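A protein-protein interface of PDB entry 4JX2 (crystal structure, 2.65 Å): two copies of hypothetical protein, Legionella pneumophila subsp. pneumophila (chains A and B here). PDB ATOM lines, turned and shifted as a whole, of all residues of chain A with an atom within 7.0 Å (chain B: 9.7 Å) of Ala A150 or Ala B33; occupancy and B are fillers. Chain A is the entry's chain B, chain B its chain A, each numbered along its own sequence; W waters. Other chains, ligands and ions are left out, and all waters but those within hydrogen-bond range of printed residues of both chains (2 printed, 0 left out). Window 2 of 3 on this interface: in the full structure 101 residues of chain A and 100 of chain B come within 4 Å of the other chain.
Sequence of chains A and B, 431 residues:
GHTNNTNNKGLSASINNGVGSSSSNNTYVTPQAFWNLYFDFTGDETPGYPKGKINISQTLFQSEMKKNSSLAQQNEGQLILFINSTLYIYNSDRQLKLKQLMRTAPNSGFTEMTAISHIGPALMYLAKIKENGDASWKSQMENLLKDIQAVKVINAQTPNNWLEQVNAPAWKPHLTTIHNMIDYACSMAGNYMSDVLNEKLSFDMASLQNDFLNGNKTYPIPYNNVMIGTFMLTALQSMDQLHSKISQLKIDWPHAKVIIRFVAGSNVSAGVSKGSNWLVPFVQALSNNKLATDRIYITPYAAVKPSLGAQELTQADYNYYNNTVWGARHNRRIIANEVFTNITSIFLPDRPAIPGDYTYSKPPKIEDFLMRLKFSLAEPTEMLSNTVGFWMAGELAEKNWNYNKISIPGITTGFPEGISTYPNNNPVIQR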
ATOM      1  N   ALA A 115      -7.673  -2.573 -16.821  1.00  0.00           N
ATOM      2  CA  ALA A 115      -6.421  -1.888 -17.138  1.00  0.00           C
ATOM      3  C   ALA A 115      -6.582  -0.370 -17.067  1.00  0.00           C
ATOM      4  O   ALA A 115      -5.706   0.314 -16.539  1.00  0.00           O
ATOM      5  CB  ALA A 115      -5.933  -2.298 -18.511  1.00  0.00           C
ATOM      6  N   LEU A 145       2.866   5.818 -19.091  1.00  0.00           N
ATOM      7  CA  LEU A 145       2.461   6.829 -20.081  1.00  0.00           C
ATOM      8  C   LEU A 145       2.594   6.269 -21.534  1.00  0.00           C
ATOM      9  O   LEU A 145       1.671   6.418 -22.338  1.00  0.00           O
ATOM     10  CB  LEU A 145       3.297   8.119 -19.886  1.00  0.00           C
ATOM     11  CG  LEU A 145       3.283   9.192 -20.989  1.00  0.00           C
ATOM     12  CD1 LEU A 145       1.900   9.607 -21.328  1.00  0.00           C
ATOM     13  CD2 LEU A 145       4.048  10.423 -20.567  1.00  0.00           C
ATOM     14  N   LYS A 146       3.715   5.600 -21.839  1.00  0.00           N
ATOM     15  CA  LYS A 146       3.961   4.973 -23.142  1.00  0.00           C
ATOM     16  C   LYS A 146       2.847   3.941 -23.494  1.00  0.00           C
ATOM     17  O   LYS A 146       2.320   3.927 -24.622  1.00  0.00           O
ATOM     18  CB  LYS A 146       5.344   4.295 -23.127  1.00  0.00           C
ATOM     19  CG  LYS A 146       5.630   3.395 -24.327  1.00  0.00           C
ATOM     20  CD  LYS A 146       6.990   2.750 -24.262  1.00  0.00           C
ATOM     21  CE  LYS A 146       7.035   1.504 -23.423  1.00  0.00           C
ATOM     22  NZ  LYS A 146       8.405   0.934 -23.438  1.00  0.00           N
ATOM     23  N   ASP A 147       2.497   3.095 -22.506  1.00  0.00           N
ATOM     24  CA  ASP A 147       1.513   2.033 -22.687  1.00  0.00           C
ATOM     25  C   ASP A 147       0.070   2.591 -22.823  1.00  0.00           C
ATOM     26  O   ASP A 147      -0.732   2.018 -23.576  1.00  0.00           O
ATOM     27  CB  ASP A 147       1.654   0.973 -21.570  1.00  0.00           C
ATOM     28  CG  ASP A 147       2.948   0.136 -21.665  1.00  0.00           C
ATOM     29  OD1 ASP A 147       3.510  -0.006 -22.798  1.00  0.00           O
ATOM     30  OD2 ASP A 147       3.377  -0.401 -20.640  1.00  0.00           O
ATOM     31  N   ILE A 148      -0.220   3.748 -22.173  1.00  0.00           N
ATOM     32  CA  ILE A 148      -1.520   4.443 -22.259  1.00  0.00           C
ATOM     33  C   ILE A 148      -1.666   5.056 -23.664  1.00  0.00           C
ATOM     34  O   ILE A 148      -2.774   5.061 -24.206  1.00  0.00           O
ATOM     35  CB  ILE A 148      -1.667   5.499 -21.123  1.00  0.00           C
ATOM     36  CG1 ILE A 148      -1.968   4.831 -19.793  1.00  0.00           C
ATOM     37  CG2 ILE A 148      -2.713   6.577 -21.424  1.00  0.00           C
ATOM     38  CD1 ILE A 148      -1.543   5.644 -18.609  1.00  0.00           C
ATOM     39  N   GLN A 149      -0.556   5.541 -24.260  1.00  0.00           N
ATOM     40  CA  GLN A 149      -0.571   6.116 -25.606  1.00  0.00           C
ATOM     41  C   GLN A 149      -0.890   5.023 -26.649  1.00  0.00           C
ATOM     42  O   GLN A 149      -1.687   5.258 -27.565  1.00  0.00           O
ATOM     43  CB  GLN A 149       0.742   6.823 -25.906  1.00  0.00           C
ATOM     44  CG  GLN A 149       0.723   7.671 -27.177  1.00  0.00           C
ATOM     45  CD  GLN A 149       1.954   8.547 -27.263  1.00  0.00           C
ATOM     46  OE1 GLN A 149       3.046   8.163 -26.821  1.00  0.00           O
ATOM     47  NE2 GLN A 149       1.805   9.752 -27.831  1.00  0.00           N
ATOM     48  N   ALA A 150      -0.323   3.816 -26.466  1.00  0.00           N
ATOM     49  CA  ALA A 150      -0.588   2.655 -27.330  1.00  0.00           C
ATOM     50  C   ALA A 150      -2.073   2.233 -27.205  1.00  0.00           C
ATOM     51  O   ALA A 150      -2.703   1.941 -28.225  1.00  0.00           O
ATOM     52  CB  ALA A 150       0.334   1.496 -26.969  1.00  0.00           C
ATOM     53  N   VAL A 151      -2.648   2.294 -25.980  1.00  0.00           N
ATOM     54  CA  VAL A 151      -4.056   1.949 -25.761  1.00  0.00           C
ATOM     55  C   VAL A 151      -4.964   2.987 -26.449  1.00  0.00           C
ATOM     56  O   VAL A 151      -5.937   2.594 -27.092  1.00  0.00           O
ATOM     57  CB  VAL A 151      -4.413   1.759 -24.270  1.00  0.00           C
ATOM     58  CG1 VAL A 151      -5.927   1.836 -24.041  1.00  0.00           C
ATOM     59  CG2 VAL A 151      -3.854   0.439 -23.745  1.00  0.00           C
ATOM     60  N   LYS A 152      -4.633   4.293 -26.345  1.00  0.00           N
ATOM     61  CA  LYS A 152      -5.435   5.345 -26.967  1.00  0.00           C
ATOM     62  C   LYS A 152      -5.577   5.075 -28.466  1.00  0.00           C
ATOM     63  O   LYS A 152      -6.683   5.166 -29.007  1.00  0.00           O
ATOM     64  CB  LYS A 152      -4.832   6.737 -26.712  1.00  0.00           C
ATOM     65  CG  LYS A 152      -5.806   7.883 -27.038  1.00  0.00           C
ATOM     66  CD  LYS A 152      -5.193   9.276 -26.888  1.00  0.00           C
ATOM     67  CE  LYS A 152      -5.951  10.331 -27.664  1.00  0.00           C
ATOM     68  NZ  LYS A 152      -7.195  10.729 -26.970  1.00  0.00           N
ATOM     69  N   VAL A 153      -4.469   4.689 -29.115  1.00  0.00           N
ATOM     70  CA  VAL A 153      -4.410   4.423 -30.550  1.00  0.00           C
ATOM     71  C   VAL A 153      -5.276   3.205 -30.901  1.00  0.00           C
ATOM     72  O   VAL A 153      -6.127   3.326 -31.783  1.00  0.00           O
ATOM     73  CB  VAL A 153      -2.939   4.271 -31.028  1.00  0.00           C
ATOM     74  CG1 VAL A 153      -2.858   3.884 -32.496  1.00  0.00           C
ATOM     75  CG2 VAL A 153      -2.161   5.554 -30.786  1.00  0.00           C
ATOM     76  N   ILE A 154      -5.094   2.066 -30.192  1.00  0.00           N
ATOM     77  CA  ILE A 154      -5.838   0.833 -30.459  1.00  0.00           C
ATOM     78  C   ILE A 154      -7.353   1.036 -30.245  1.00  0.00           C
ATOM     79  O   ILE A 154      -8.155   0.517 -31.034  1.00  0.00           O
ATOM     80  CB  ILE A 154      -5.265  -0.367 -29.662  1.00  0.00           C
ATOM     81  CG1 ILE A 154      -5.448  -1.675 -30.415  1.00  0.00           C
ATOM     82  CG2 ILE A 154      -5.820  -0.493 -28.278  1.00  0.00           C
ATOM     83  CD1 ILE A 154      -4.275  -2.056 -31.304  1.00  0.00           C
ATOM     84  N   ASN A 155      -7.730   1.832 -29.228  1.00  0.00           N
ATOM     85  CA  ASN A 155      -9.123   2.155 -28.903  1.00  0.00           C
ATOM     86  C   ASN A 155      -9.759   3.003 -30.009  1.00  0.00           C
ATOM     87  O   ASN A 155     -10.975   2.954 -30.195  1.00  0.00           O
ATOM     88  CB  ASN A 155      -9.204   2.893 -27.561  1.00  0.00           C
ATOM     89  CG  ASN A 155     -10.607   3.098 -27.054  1.00  0.00           C
ATOM     90  OD1 ASN A 155     -11.259   2.171 -26.580  1.00  0.00           O
ATOM     91  ND2 ASN A 155     -11.087   4.330 -27.113  1.00  0.00           N
ATOM     92  N   ALA A 156      -8.942   3.774 -30.743  1.00  0.00           N
ATOM     93  CA  ALA A 156      -9.445   4.624 -31.812  1.00  0.00           C
ATOM     94  C   ALA A 156      -9.557   3.864 -33.160  1.00  0.00           C
ATOM     95  O   ALA A 156     -10.123   4.417 -34.113  1.00  0.00           O
ATOM     96  CB  ALA A 156      -8.567   5.850 -31.954  1.00  0.00           C
ATOM     97  N   CYS A 186      -7.384   8.020 -21.505  1.00  0.00           N
ATOM     98  CA  CYS A 186      -6.013   7.969 -22.014  1.00  0.00           C
ATOM     99  C   CYS A 186      -5.444   9.361 -22.196  1.00  0.00           C
ATOM    100  O   CYS A 186      -4.320   9.622 -21.765  1.00  0.00           O
ATOM    101  CB  CYS A 186      -5.940   7.160 -23.300  1.00  0.00           C
ATOM    102  SG  CYS A 186      -6.326   5.402 -23.081  1.00  0.00           S
ATOM    103  N   ILE A 429      -1.909  12.776 -26.693  1.00  0.00           N
ATOM    104  CA  ILE A 429      -0.961  12.757 -25.585  1.00  0.00           C
ATOM    105  C   ILE A 429       0.359  13.377 -26.102  1.00  0.00           C
ATOM    106  O   ILE A 429       0.984  12.835 -27.023  1.00  0.00           O
ATOM    107  CB  ILE A 429      -0.786  11.326 -24.982  1.00  0.00           C
ATOM    108  CG1 ILE A 429      -2.127  10.781 -24.428  1.00  0.00           C
ATOM    109  CG2 ILE A 429       0.320  11.321 -23.914  1.00  0.00           C
ATOM    110  CD1 ILE A 429      -2.271   9.283 -24.451  1.00  0.00           C
ATOM    111  N   VAL B  29      -9.569 -11.624 -29.477  1.00  0.00           N
ATOM    112  CA  VAL B  29      -8.312 -11.583 -28.746  1.00  0.00           C
ATOM    113  C   VAL B  29      -8.165 -10.186 -28.165  1.00  0.00           C
ATOM    114  O   VAL B  29      -8.232  -9.207 -28.910  1.00  0.00           O
ATOM    115  CB  VAL B  29      -7.104 -11.963 -29.656  1.00  0.00           C
ATOM    116  CG1 VAL B  29      -5.776 -11.733 -28.945  1.00  0.00           C
ATOM    117  CG2 VAL B  29      -7.201 -13.403 -30.155  1.00  0.00           C
ATOM    118  N   THR B  30      -7.967 -10.090 -26.845  1.00  0.00           N
ATOM    119  CA  THR B  30      -7.706  -8.819 -26.179  1.00  0.00           C
ATOM    120  C   THR B  30      -6.445  -8.181 -26.804  1.00  0.00           C
ATOM    121  O   THR B  30      -5.391  -8.841 -26.824  1.00  0.00           O
ATOM    122  CB  THR B  30      -7.535  -9.029 -24.661  1.00  0.00           C
ATOM    123  OG1 THR B  30      -8.806  -9.290 -24.065  1.00  0.00           O
ATOM    124  CG2 THR B  30      -6.889  -7.838 -23.964  1.00  0.00           C
ATOM    125  N   PRO B  31      -6.551  -6.921 -27.325  1.00  0.00           N
ATOM    126  CA  PRO B  31      -5.364  -6.242 -27.886  1.00  0.00           C
ATOM    127  C   PRO B  31      -4.187  -6.229 -26.909  1.00  0.00           C
ATOM    128  O   PRO B  31      -4.376  -6.036 -25.705  1.00  0.00           O
ATOM    129  CB  PRO B  31      -5.863  -4.822 -28.162  1.00  0.00           C
ATOM    130  CG  PRO B  31      -7.342  -4.971 -28.327  1.00  0.00           C
ATOM    131  CD  PRO B  31      -7.744  -6.043 -27.367  1.00  0.00           C
ATOM    132  N   GLN B  32      -2.964  -6.468 -27.429  1.00  0.00           N
ATOM    133  CA  GLN B  32      -1.739  -6.522 -26.630  1.00  0.00           C
ATOM    134  C   GLN B  32      -1.519  -5.243 -25.807  1.00  0.00           C
ATOM    135  O   GLN B  32      -1.070  -5.339 -24.665  1.00  0.00           O
ATOM    136  CB  GLN B  32      -0.525  -6.795 -27.523  1.00  0.00           C
ATOM    137  CG  GLN B  32       0.766  -7.107 -26.762  1.00  0.00           C
ATOM    138  CD  GLN B  32       0.666  -8.346 -25.919  1.00  0.00           C
ATOM    139  OE1 GLN B  32       0.322  -9.431 -26.406  1.00  0.00           O
ATOM    140  NE2 GLN B  32       0.978  -8.202 -24.631  1.00  0.00           N
ATOM    141  N   ALA B  33      -1.843  -4.063 -26.371  1.00  0.00           N
ATOM    142  CA  ALA B  33      -1.707  -2.793 -25.667  1.00  0.00           C
ATOM    143  C   ALA B  33      -2.449  -2.843 -24.336  1.00  0.00           C
ATOM    144  O   ALA B  33      -1.910  -2.365 -23.337  1.00  0.00           O
ATOM    145  CB  ALA B  33      -2.217  -1.645 -26.520  1.00  0.00           C
ATOM    146  N   PHE B  34      -3.650  -3.484 -24.296  1.00  0.00           N
ATOM    147  CA  PHE B  34      -4.422  -3.605 -23.053  1.00  0.00           C
ATOM    148  C   PHE B  34      -3.717  -4.517 -22.026  1.00  0.00           C
ATOM    149  O   PHE B  34      -3.682  -4.181 -20.846  1.00  0.00           O
ATOM    150  CB  PHE B  34      -5.845  -4.080 -23.305  1.00  0.00           C
ATOM    151  CG  PHE B  34      -6.775  -3.002 -23.801  1.00  0.00           C
ATOM    152  CD1 PHE B  34      -7.166  -1.959 -22.968  1.00  0.00           C
ATOM    153  CD2 PHE B  34      -7.300  -3.049 -25.087  1.00  0.00           C
ATOM    154  CE1 PHE B  34      -8.060  -0.983 -23.415  1.00  0.00           C
ATOM    155  CE2 PHE B  34      -8.193  -2.076 -25.529  1.00  0.00           C
ATOM    156  CZ  PHE B  34      -8.572  -1.052 -24.686  1.00  0.00           C
ATOM    157  N   TRP B  35      -3.138  -5.631 -22.463  1.00  0.00           N
ATOM    158  CA  TRP B  35      -2.408  -6.512 -21.564  1.00  0.00           C
ATOM    159  C   TRP B  35      -1.194  -5.791 -20.996  1.00  0.00           C
ATOM    160  O   TRP B  35      -0.964  -5.841 -19.790  1.00  0.00           O
ATOM    161  CB  TRP B  35      -1.983  -7.797 -22.282  1.00  0.00           C
ATOM    162  CG  TRP B  35      -3.011  -8.892 -22.276  1.00  0.00           C
ATOM    163  CD1 TRP B  35      -3.573  -9.488 -23.367  1.00  0.00           C
ATOM    164  CD2 TRP B  35      -3.566  -9.556 -21.123  1.00  0.00           C
ATOM    165  NE1 TRP B  35      -4.448 -10.483 -22.971  1.00  0.00           N
ATOM    166  CE2 TRP B  35      -4.473 -10.536 -21.599  1.00  0.00           C
ATOM    167  CE3 TRP B  35      -3.382  -9.423 -19.728  1.00  0.00           C
ATOM    168  CZ2 TRP B  35      -5.180 -11.386 -20.737  1.00  0.00           C
ATOM    169  CZ3 TRP B  35      -4.091 -10.260 -18.875  1.00  0.00           C
ATOM    170  CH2 TRP B  35      -4.984 -11.221 -19.379  1.00  0.00           C
ATOM    171  N   ASN B  36      -0.452  -5.074 -21.850  1.00  0.00           N
ATOM    172  CA  ASN B  36       0.720  -4.298 -21.438  1.00  0.00           C
ATOM    173  C   ASN B  36       0.339  -3.307 -20.326  1.00  0.00           C
ATOM    174  O   ASN B  36       1.001  -3.295 -19.286  1.00  0.00           O
ATOM    175  CB  ASN B  36       1.367  -3.583 -22.633  1.00  0.00           C
ATOM    176  CG  ASN B  36       1.919  -4.523 -23.685  1.00  0.00           C
ATOM    177  OD1 ASN B  36       1.966  -5.749 -23.516  1.00  0.00           O
ATOM    178  ND2 ASN B  36       2.346  -3.967 -24.802  1.00  0.00           N
ATOM    179  N   LEU B  37      -0.774  -2.557 -20.507  1.00  0.00           N
ATOM    180  CA  LEU B  37      -1.278  -1.607 -19.519  1.00  0.00           C
ATOM    181  C   LEU B  37      -1.707  -2.336 -18.253  1.00  0.00           C
ATOM    182  O   LEU B  37      -1.390  -1.871 -17.156  1.00  0.00           O
ATOM    183  CB  LEU B  37      -2.446  -0.759 -20.077  1.00  0.00           C
ATOM    184  CG  LEU B  37      -3.007   0.332 -19.132  1.00  0.00           C
ATOM    185  CD1 LEU B  37      -1.920   1.331 -18.736  1.00  0.00           C
ATOM    186  CD2 LEU B  37      -4.189   1.042 -19.737  1.00  0.00           C
ATOM    187  N   TYR B  38      -2.401  -3.480 -18.402  1.00  0.00           N
ATOM    188  CA  TYR B  38      -2.872  -4.290 -17.281  1.00  0.00           C
ATOM    189  C   TYR B  38      -1.705  -4.724 -16.380  1.00  0.00           C
ATOM    190  O   TYR B  38      -1.726  -4.476 -15.172  1.00  0.00           O
ATOM    191  CB  TYR B  38      -3.665  -5.518 -17.767  1.00  0.00           C
ATOM    192  CG  TYR B  38      -4.223  -6.338 -16.625  1.00  0.00           C
ATOM    193  CD1 TYR B  38      -5.360  -5.926 -15.937  1.00  0.00           C
ATOM    194  CD2 TYR B  38      -3.579  -7.494 -16.190  1.00  0.00           C
ATOM    195  CE1 TYR B  38      -5.854  -6.654 -14.856  1.00  0.00           C
ATOM    196  CE2 TYR B  38      -4.063  -8.229 -15.106  1.00  0.00           C
ATOM    197  CZ  TYR B  38      -5.211  -7.815 -14.455  1.00  0.00           C
ATOM    198  OH  TYR B  38      -5.680  -8.533 -13.383  1.00  0.00           O
ATOM    199  N   PHE B  39      -0.666  -5.300 -16.991  1.00  0.00           N
ATOM    200  CA  PHE B  39       0.511  -5.827 -16.317  1.00  0.00           C
ATOM    201  C   PHE B  39       1.439  -4.748 -15.748  1.00  0.00           C
ATOM    202  O   PHE B  39       2.326  -5.089 -14.961  1.00  0.00           O
ATOM    203  CB  PHE B  39       1.276  -6.754 -17.262  1.00  0.00           C
ATOM    204  CG  PHE B  39       0.598  -8.085 -17.499  1.00  0.00           C
ATOM    205  CD1 PHE B  39       0.011  -8.782 -16.452  1.00  0.00           C
ATOM    206  CD2 PHE B  39       0.569  -8.652 -18.767  1.00  0.00           C
ATOM    207  CE1 PHE B  39      -0.598 -10.011 -16.673  1.00  0.00           C
ATOM    208  CE2 PHE B  39      -0.010  -9.900 -18.978  1.00  0.00           C
ATOM    209  CZ  PHE B  39      -0.591 -10.570 -17.931  1.00  0.00           C
ATOM    210  N   ASP B  40       1.210  -3.459 -16.083  1.00  0.00           N
ATOM    211  CA  ASP B  40       1.973  -2.327 -15.545  1.00  0.00           C
ATOM    212  C   ASP B  40       1.666  -2.107 -14.065  1.00  0.00           C
ATOM    213  O   ASP B  40       2.520  -1.610 -13.334  1.00  0.00           O
ATOM    214  CB  ASP B  40       1.679  -1.029 -16.327  1.00  0.00           C
ATOM    215  CG  ASP B  40       2.359  -0.901 -17.688  1.00  0.00           C
ATOM    216  OD1 ASP B  40       3.427  -1.529 -17.891  1.00  0.00           O
ATOM    217  OD2 ASP B  40       1.841  -0.169 -18.530  1.00  0.00           O
HETATM  218  O   HOH W   1      -3.357  -0.858 -15.438  1.00  0.00           O
HETATM  219  O   HOH W   2       0.059  -0.702 -23.930  1.00  0.00           O
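The side-chain carboxylate (OD2) of Asp B40 lies close to the side-chain carboxylate (OD2) of Asp A147 (2.6 Å).
NE2 of Gln B32 sits at hydrogen-bond distance from OD1 of Asn B36, 2.9 Å away. O of Ile A148 sits at hydrogen-bond distance from SG of Cys A186 (3.7 Å).
CB of Ala A115 touches O of Phe B34 (3.8 Å). Ala A115 touches Leu B37 (O to CD2, 3.6 Å). Tyr B38 touches Ala A115 (N to CB, 3.7 Å). O of Asn B36 touches OD2 of Asp A147 (3.98 Å). CD1 of Leu B37 touches CG1 of Ile A148, at 3.7 Å. C of Ala A150 touches CB of Ala B33, at 3.9 Å. Val A151 touches Ala B33. CG1 of Val A151 touches CE1 of Phe B34, 3.6 Å away. Ile A154 touches Pro B31 (CG1 to CB, 3.9 Å). Ile A154 touches Phe B34 (CG2 to CE2, 3.96 Å).
Ala B33 touches two residues of chain A. Of chain B, only Ala B33 and Phe B34 come within 4 Å of Val A151. No residue of chain B comes within 4 Å of Val A153. Of the printed residues of chain A, Asp B40 touches Asp A147 (2.6 Å). Of the printed residues of chain A, Tyr B38 touches Ala A115. Cys A186 touches none of the printed residues of chain B. Ala A156 touches none of the printed residues of chain B. The nearest residue of chain B that does not touch Ala A150 is Asn B36 (6.2 Å). The nearest residue of chain A that does not touch Ala B33 is Ile A154 (4.2 Å). The nearest printed residue of chain A that does not touch Phe B34 is Asn A155 (4.6 Å).
Hydrophobic or aromatic side chains of chain A that line the printed part of chain B: Ala A115, Ile A148, Val A151 and Ile A154. Printed residues of chain B that touch a printed residue of chain A: Pro B31, Ala B33, Phe B34, Asn B36, Leu B37, Tyr B38 and Asp B40. Hydrophobic or aromatic side chains of chain B within 4 Å of the printed part of chain A: Pro B31, Ala B33, Phe B34 and Leu B37. Among the printed residues, 11 pairs touch across the chains. Among the printed residues, no Asp or Glu carboxylate lies within 4 Å of a Lys or Arg side-chain nitrogen of the other chain.
No position is printed for both chains. Of the 11 pairs that touch across the chains among the printed residues, none has its exchanged pair printed and touching as well.
Water W2 bridges O of Ala B33 (2.6 Å) and O of Asp A147 (2.9 Å). Water W1 bridges the backbone carbonyl oxygen of Leu B37 (2.8 Å) and the backbone carbonyl oxygen of Ala A115 (2.8 Å).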
